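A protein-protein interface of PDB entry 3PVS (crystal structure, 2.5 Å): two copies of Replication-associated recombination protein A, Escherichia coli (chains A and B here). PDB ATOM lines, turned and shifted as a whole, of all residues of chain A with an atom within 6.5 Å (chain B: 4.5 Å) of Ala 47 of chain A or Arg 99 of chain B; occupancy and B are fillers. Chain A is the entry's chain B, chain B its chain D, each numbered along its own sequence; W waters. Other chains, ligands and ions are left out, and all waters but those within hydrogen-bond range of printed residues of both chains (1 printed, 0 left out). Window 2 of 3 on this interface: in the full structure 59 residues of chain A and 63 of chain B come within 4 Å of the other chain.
Arg 99 of chain B touches just these residues of chain A: Glu 46 (3.0 Å) and Ala 47 (3.6 Å).
Of the printed residues of chain A, Gln 100 of chain B touches Tyr 73.
Of the printed residues of chain B, Glu 46 of chain A touches Glu 96 (2.6 Å), Arg 99 (3.0 Å) and Asn 103 (2.9 Å).
Of the printed residues of chain B, Tyr 73 of chain A touches Glu 96 (2.5 Å), Gln 100 (3.6 Å) and Asn 103 (3.1 Å).
The nearest residue of chain A that does not touch Arg 99 of chain B is Tyr 73 of chain A (4.5 Å).
O of Glu 46 of chain A sits at hydrogen-bond distance from ND2 of Asn 103 of chain B (2.9 Å).
NH2 of Arg 99 of chain B sits at hydrogen-bond distance from O of Glu 46 of chain A, at 3.0 Å.
The side-chain carboxylate of Glu 46 of chain A sits close to the side-chain carboxylate of Glu 96 of chain B (2.6 Å).
The backbone carbonyl oxygen (O) of Tyr 73 of chain A is in hydrogen-bond range of the side-chain amide nitrogen (ND2) of Asn 103 of chain B (3.1 Å).
The side-chain carboxylate (OE2) of Glu 96 of chain B lies within hydrogen-bond range of the side-chain hydroxyl (OH) of Tyr 73 of chain A (2.5 Å).
Among the printed residues, pairs that only touch across the chains: Ala 47 of chain A with Arg 99 of chain B (3.6 Å), Ala 47 of chain A with Asn 103 of chain B (3.9 Å), Gly 48 of chain A with Asn 103 of chain B (3.96 Å) and Tyr 73 of chain A with Gln 100 of chain B (3.6 Å).
Water W1 bridges OE2 of Glu 46 of chain A (2.9 Å) and OE1 of Glu 96 of chain B (3.2 Å).
Along chain A the printed residues that touch a printed residue of chain B span positions 46 to 73.
No position is printed for both chains.
OD1 of Asn 103 of chain B is in hydrogen-bond range of NE of Arg 99 of chain B, at 3.3 Å.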
ATOM      1  N   PRO A  42     -29.084  25.138  -6.607  1.00  0.00           N
ATOM      2  CA  PRO A  42     -28.664  24.001  -7.398  1.00  0.00           C
ATOM      3  C   PRO A  42     -28.177  24.476  -8.751  1.00  0.00           C
ATOM      4  O   PRO A  42     -27.113  24.050  -9.213  1.00  0.00           O
ATOM      5  CB  PRO A  42     -29.951  23.193  -7.593  1.00  0.00           C
ATOM      6  CG  PRO A  42     -30.804  23.566  -6.510  1.00  0.00           C
ATOM      7  CD  PRO A  42     -30.456  24.961  -6.101  1.00  0.00           C
ATOM      8  N   ARG A  43     -28.924  25.390  -9.361  1.00  0.00           N
ATOM      9  CA  ARG A  43     -28.607  25.824 -10.708  1.00  0.00           C
ATOM     10  C   ARG A  43     -27.291  26.576 -10.810  1.00  0.00           C
ATOM     11  O   ARG A  43     -26.572  26.380 -11.772  1.00  0.00           O
ATOM     12  CB  ARG A  43     -29.774  26.589 -11.329  1.00  0.00           C
ATOM     13  CG  ARG A  43     -30.784  25.621 -11.975  1.00  0.00           C
ATOM     14  CD  ARG A  43     -32.238  26.147 -11.933  1.00  0.00           C
ATOM     15  NE  ARG A  43     -32.532  27.195 -12.918  1.00  0.00           N
ATOM     16  CZ  ARG A  43     -32.654  26.993 -14.237  1.00  0.00           C
ATOM     17  NH1 ARG A  43     -32.493  25.776 -14.767  1.00  0.00           N
ATOM     18  NH2 ARG A  43     -32.929  28.021 -15.041  1.00  0.00           N
ATOM     19  N   ALA A  44     -26.953  27.414  -9.837  1.00  0.00           N
ATOM     20  CA  ALA A  44     -25.665  28.095  -9.906  1.00  0.00           C
ATOM     21  C   ALA A  44     -24.487  27.139  -9.652  1.00  0.00           C
ATOM     22  O   ALA A  44     -23.393  27.299 -10.231  1.00  0.00           O
ATOM     23  CB  ALA A  44     -25.617  29.270  -8.961  1.00  0.00           C
ATOM     24  N   ILE A  45     -24.720  26.161  -8.772  1.00  0.00           N
ATOM     25  CA  ILE A  45     -23.750  25.120  -8.460  1.00  0.00           C
ATOM     26  C   ILE A  45     -23.501  24.291  -9.718  1.00  0.00           C
ATOM     27  O   ILE A  45     -22.365  24.128 -10.173  1.00  0.00           O
ATOM     28  CB  ILE A  45     -24.257  24.229  -7.278  1.00  0.00           C
ATOM     29  CG1 ILE A  45     -24.181  25.011  -5.945  1.00  0.00           C
ATOM     30  CG2 ILE A  45     -23.436  22.950  -7.166  1.00  0.00           C
ATOM     31  CD1 ILE A  45     -24.942  24.400  -4.774  1.00  0.00           C
ATOM     32  N   GLU A  46     -24.601  23.808 -10.278  1.00  0.00           N
ATOM     33  CA  GLU A  46     -24.634  23.013 -11.488  1.00  0.00           C
ATOM     34  C   GLU A  46     -23.843  23.716 -12.580  1.00  0.00           C
ATOM     35  O   GLU A  46     -23.113  23.070 -13.337  1.00  0.00           O
ATOM     36  CB  GLU A  46     -26.090  22.895 -11.919  1.00  0.00           C
ATOM     37  CG  GLU A  46     -26.486  21.642 -12.616  1.00  0.00           C
ATOM     38  CD  GLU A  46     -26.255  20.424 -11.758  1.00  0.00           C
ATOM     39  OE1 GLU A  46     -26.966  20.246 -10.740  1.00  0.00           O
ATOM     40  OE2 GLU A  46     -25.362  19.636 -12.138  1.00  0.00           O
ATOM     41  N   ALA A  47     -23.971  25.040 -12.662  1.00  0.00           N
ATOM     42  CA  ALA A  47     -23.234  25.809 -13.672  1.00  0.00           C
ATOM     43  C   ALA A  47     -21.800  26.064 -13.227  1.00  0.00           C
ATOM     44  O   ALA A  47     -20.980  26.528 -14.008  1.00  0.00           O
ATOM     45  CB  ALA A  47     -23.949  27.125 -13.970  1.00  0.00           C
ATOM     46  N   GLY A  48     -21.518  25.777 -11.950  1.00  0.00           N
ATOM     47  CA  GLY A  48     -20.198  26.008 -11.365  1.00  0.00           C
ATOM     48  C   GLY A  48     -19.840  27.480 -11.339  1.00  0.00           C
ATOM     49  O   GLY A  48     -18.693  27.850 -11.555  1.00  0.00           O
ATOM     50  N   HIS A  49     -20.834  28.325 -11.098  1.00  0.00           N
ATOM     51  CA  HIS A  49     -20.603  29.756 -11.054  1.00  0.00           C
ATOM     52  C   HIS A  49     -20.319  30.029  -9.611  1.00  0.00           C
ATOM     53  O   HIS A  49     -21.020  29.512  -8.749  1.00  0.00           O
ATOM     54  CB  HIS A  49     -21.822  30.521 -11.587  1.00  0.00           C
ATOM     55  CG  HIS A  49     -21.913  30.546 -13.096  1.00  0.00           C
ATOM     56  ND1 HIS A  49     -20.800  30.613 -13.920  1.00  0.00           N
ATOM     57  CD2 HIS A  49     -22.990  30.544 -13.928  1.00  0.00           C
ATOM     58  CE1 HIS A  49     -21.189  30.632 -15.187  1.00  0.00           C
ATOM     59  NE2 HIS A  49     -22.513  30.595 -15.221  1.00  0.00           N
ATOM     60  N   TYR A  73     -18.110  20.982  -8.515  1.00  0.00           N
ATOM     61  CA  TYR A  73     -18.792  21.516  -9.698  1.00  0.00           C
ATOM     62  C   TYR A  73     -18.053  22.685 -10.340  1.00  0.00           C
ATOM     63  O   TYR A  73     -18.164  22.912 -11.542  1.00  0.00           O
ATOM     64  CB  TYR A  73     -20.198  21.980  -9.363  1.00  0.00           C
ATOM     65  CG  TYR A  73     -21.165  20.852  -9.248  1.00  0.00           C
ATOM     66  CD1 TYR A  73     -21.788  20.326 -10.370  1.00  0.00           C
ATOM     67  CD2 TYR A  73     -21.439  20.274  -8.003  1.00  0.00           C
ATOM     68  CE1 TYR A  73     -22.665  19.276 -10.256  1.00  0.00           C
ATOM     69  CE2 TYR A  73     -22.316  19.224  -7.883  1.00  0.00           C
ATOM     70  CZ  TYR A  73     -22.935  18.739  -9.007  1.00  0.00           C
ATOM     71  OH  TYR A  73     -23.800  17.681  -8.875  1.00  0.00           O
ATOM     72  N   ALA A  74     -17.316  23.437  -9.547  1.00  0.00           N
ATOM     73  CA  ALA A  74     -16.671  24.608 -10.085  1.00  0.00           C
ATOM     74  C   ALA A  74     -15.255  24.300 -10.463  1.00  0.00           C
ATOM     75  O   ALA A  74     -14.511  25.201 -10.856  1.00  0.00           O
ATOM     76  CB  ALA A  74     -16.704  25.732  -9.067  1.00  0.00           C
ATOM     77  N   ILE B  95     -25.078  11.163 -14.403  1.00  0.00           N
ATOM     78  CA  ILE B  95     -25.377  12.487 -14.924  1.00  0.00           C
ATOM     79  C   ILE B  95     -24.567  13.592 -14.230  1.00  0.00           C
ATOM     80  O   ILE B  95     -23.871  14.358 -14.897  1.00  0.00           O
ATOM     81  CB  ILE B  95     -26.894  12.777 -14.897  1.00  0.00           C
ATOM     82  CG1 ILE B  95     -27.577  11.938 -15.974  1.00  0.00           C
ATOM     83  CG2 ILE B  95     -27.183  14.245 -15.130  1.00  0.00           C
ATOM     84  CD1 ILE B  95     -29.102  11.753 -15.742  1.00  0.00           C
ATOM     85  N   GLU B  96     -24.621  13.634 -12.900  1.00  0.00           N
ATOM     86  CA  GLU B  96     -23.963  14.694 -12.173  1.00  0.00           C
ATOM     87  C   GLU B  96     -22.454  14.652 -12.407  1.00  0.00           C
ATOM     88  O   GLU B  96     -21.801  15.695 -12.450  1.00  0.00           O
ATOM     89  CB  GLU B  96     -24.301  14.618 -10.684  1.00  0.00           C
ATOM     90  CG  GLU B  96     -25.719  15.113 -10.341  1.00  0.00           C
ATOM     91  CD  GLU B  96     -26.072  16.456 -11.020  1.00  0.00           C
ATOM     92  OE1 GLU B  96     -26.921  16.464 -11.941  1.00  0.00           O
ATOM     93  OE2 GLU B  96     -25.484  17.504 -10.648  1.00  0.00           O
ATOM     94  N   ARG B  97     -21.908  13.448 -12.588  1.00  0.00           N
ATOM     95  CA  ARG B  97     -20.472  13.268 -12.691  1.00  0.00           C
ATOM     96  C   ARG B  97     -20.007  13.829 -14.055  1.00  0.00           C
ATOM     97  O   ARG B  97     -18.948  14.498 -14.168  1.00  0.00           O
ATOM     98  CB  ARG B  97     -20.149  11.773 -12.586  1.00  0.00           C
ATOM     99  CG  ARG B  97     -18.883  11.398 -11.830  1.00  0.00           C
ATOM    100  CD  ARG B  97     -17.902  12.589 -11.742  1.00  0.00           C
ATOM    101  NE  ARG B  97     -16.487  12.242 -11.861  1.00  0.00           N
ATOM    102  CZ  ARG B  97     -15.532  13.077 -12.273  1.00  0.00           C
ATOM    103  NH1 ARG B  97     -15.836  14.330 -12.604  1.00  0.00           N
ATOM    104  NH2 ARG B  97     -14.264  12.650 -12.349  1.00  0.00           N
ATOM    105  N   ALA B  98     -20.831  13.551 -15.076  1.00  0.00           N
ATOM    106  CA  ALA B  98     -20.638  14.093 -16.424  1.00  0.00           C
ATOM    107  C   ALA B  98     -20.676  15.596 -16.342  1.00  0.00           C
ATOM    108  O   ALA B  98     -19.868  16.308 -16.974  1.00  0.00           O
ATOM    109  CB  ALA B  98     -21.726  13.610 -17.353  1.00  0.00           C
ATOM    110  N   ARG B  99     -21.588  16.081 -15.510  1.00  0.00           N
ATOM    111  CA  ARG B  99     -21.742  17.500 -15.369  1.00  0.00           C
ATOM    112  C   ARG B  99     -20.483  18.138 -14.823  1.00  0.00           C
ATOM    113  O   ARG B  99     -20.067  19.150 -15.323  1.00  0.00           O
ATOM    114  CB  ARG B  99     -22.967  17.835 -14.531  1.00  0.00           C
ATOM    115  CG  ARG B  99     -23.776  19.032 -15.057  1.00  0.00           C
ATOM    116  CD  ARG B  99     -23.006  19.851 -16.145  1.00  0.00           C
ATOM    117  NE  ARG B  99     -23.056  21.307 -15.967  1.00  0.00           N
ATOM    118  CZ  ARG B  99     -24.091  22.064 -16.322  1.00  0.00           C
ATOM    119  NH1 ARG B  99     -25.168  21.497 -16.854  1.00  0.00           N
ATOM    120  NH2 ARG B  99     -24.052  23.384 -16.140  1.00  0.00           N
ATOM    121  N   GLN B 100     -19.850  17.551 -13.815  1.00  0.00           N
ATOM    122  CA  GLN B 100     -18.632  18.153 -13.273  1.00  0.00           C
ATOM    123  C   GLN B 100     -17.497  18.019 -14.250  1.00  0.00           C
ATOM    124  O   GLN B 100     -16.595  18.873 -14.363  1.00  0.00           O
ATOM    125  CB  GLN B 100     -18.239  17.495 -11.962  1.00  0.00           C
ATOM    126  CG  GLN B 100     -19.382  17.480 -10.969  1.00  0.00           C
ATOM    127  CD  GLN B 100     -18.999  16.826  -9.669  1.00  0.00           C
ATOM    128  OE1 GLN B 100     -18.560  15.681  -9.649  1.00  0.00           O
ATOM    129  NE2 GLN B 100     -19.169  17.551  -8.579  1.00  0.00           N
ATOM    130  N   ASN B 101     -17.514  16.919 -14.964  1.00  0.00           N
ATOM    131  CA  ASN B 101     -16.456  16.735 -15.901  1.00  0.00           C
ATOM    132  C   ASN B 101     -16.502  17.780 -17.060  1.00  0.00           C
ATOM    133  O   ASN B 101     -15.481  18.314 -17.497  1.00  0.00           O
ATOM    134  CB  ASN B 101     -16.433  15.288 -16.337  1.00  0.00           C
ATOM    135  CG  ASN B 101     -15.089  14.881 -16.803  1.00  0.00           C
ATOM    136  OD1 ASN B 101     -14.068  15.336 -16.263  1.00  0.00           O
ATOM    137  ND2 ASN B 101     -15.053  14.074 -17.869  1.00  0.00           N
ATOM    138  N   ARG B 102     -17.717  18.115 -17.470  1.00  0.00           N
ATOM    139  CA  ARG B 102     -17.982  19.186 -18.399  1.00  0.00           C
ATOM    140  C   ARG B 102     -17.542  20.535 -17.837  1.00  0.00           C
ATOM    141  O   ARG B 102     -16.958  21.351 -18.552  1.00  0.00           O
ATOM    142  CB  ARG B 102     -19.467  19.205 -18.787  1.00  0.00           C
ATOM    143  CG  ARG B 102     -19.903  20.522 -19.404  1.00  0.00           C
ATOM    144  CD  ARG B 102     -21.360  20.576 -19.679  1.00  0.00           C
ATOM    145  NE  ARG B 102     -21.756  21.886 -20.209  1.00  0.00           N
ATOM    146  CZ  ARG B 102     -22.837  22.081 -20.962  1.00  0.00           C
ATOM    147  NH1 ARG B 102     -23.626  21.047 -21.280  1.00  0.00           N
ATOM    148  NH2 ARG B 102     -23.122  23.307 -21.386  1.00  0.00           N
ATOM    149  N   ASN B 103     -17.780  20.774 -16.557  1.00  0.00           N
ATOM    150  CA  ASN B 103     -17.324  22.057 -15.962  1.00  0.00           C
ATOM    151  C   ASN B 103     -15.827  22.218 -15.790  1.00  0.00           C
ATOM    152  O   ASN B 103     -15.346  23.333 -15.574  1.00  0.00           O
ATOM    153  CB  ASN B 103     -18.044  22.353 -14.648  1.00  0.00           C
ATOM    154  CG  ASN B 103     -19.549  22.531 -14.837  1.00  0.00           C
ATOM    155  OD1 ASN B 103     -20.030  22.695 -15.956  1.00  0.00           O
ATOM    156  ND2 ASN B 103     -20.293  22.465 -13.744  1.00  0.00           N
ATOM    157  N   THR B 134     -23.624  17.842 -22.635  1.00  0.00           N
ATOM    158  CA  THR B 134     -22.917  17.290 -21.478  1.00  0.00           C
ATOM    159  C   THR B 134     -22.339  15.881 -21.733  1.00  0.00           C
ATOM    160  O   THR B 134     -21.208  15.585 -21.309  1.00  0.00           O
ATOM    161  CB  THR B 134     -23.799  17.303 -20.213  1.00  0.00           C
ATOM    162  OG1 THR B 134     -24.188  18.650 -19.950  1.00  0.00           O
ATOM    163  CG2 THR B 134     -23.035  16.848 -19.018  1.00  0.00           C
HETATM  164  O   HOH W   1     -27.448  18.806 -14.033  1.00  0.00           O
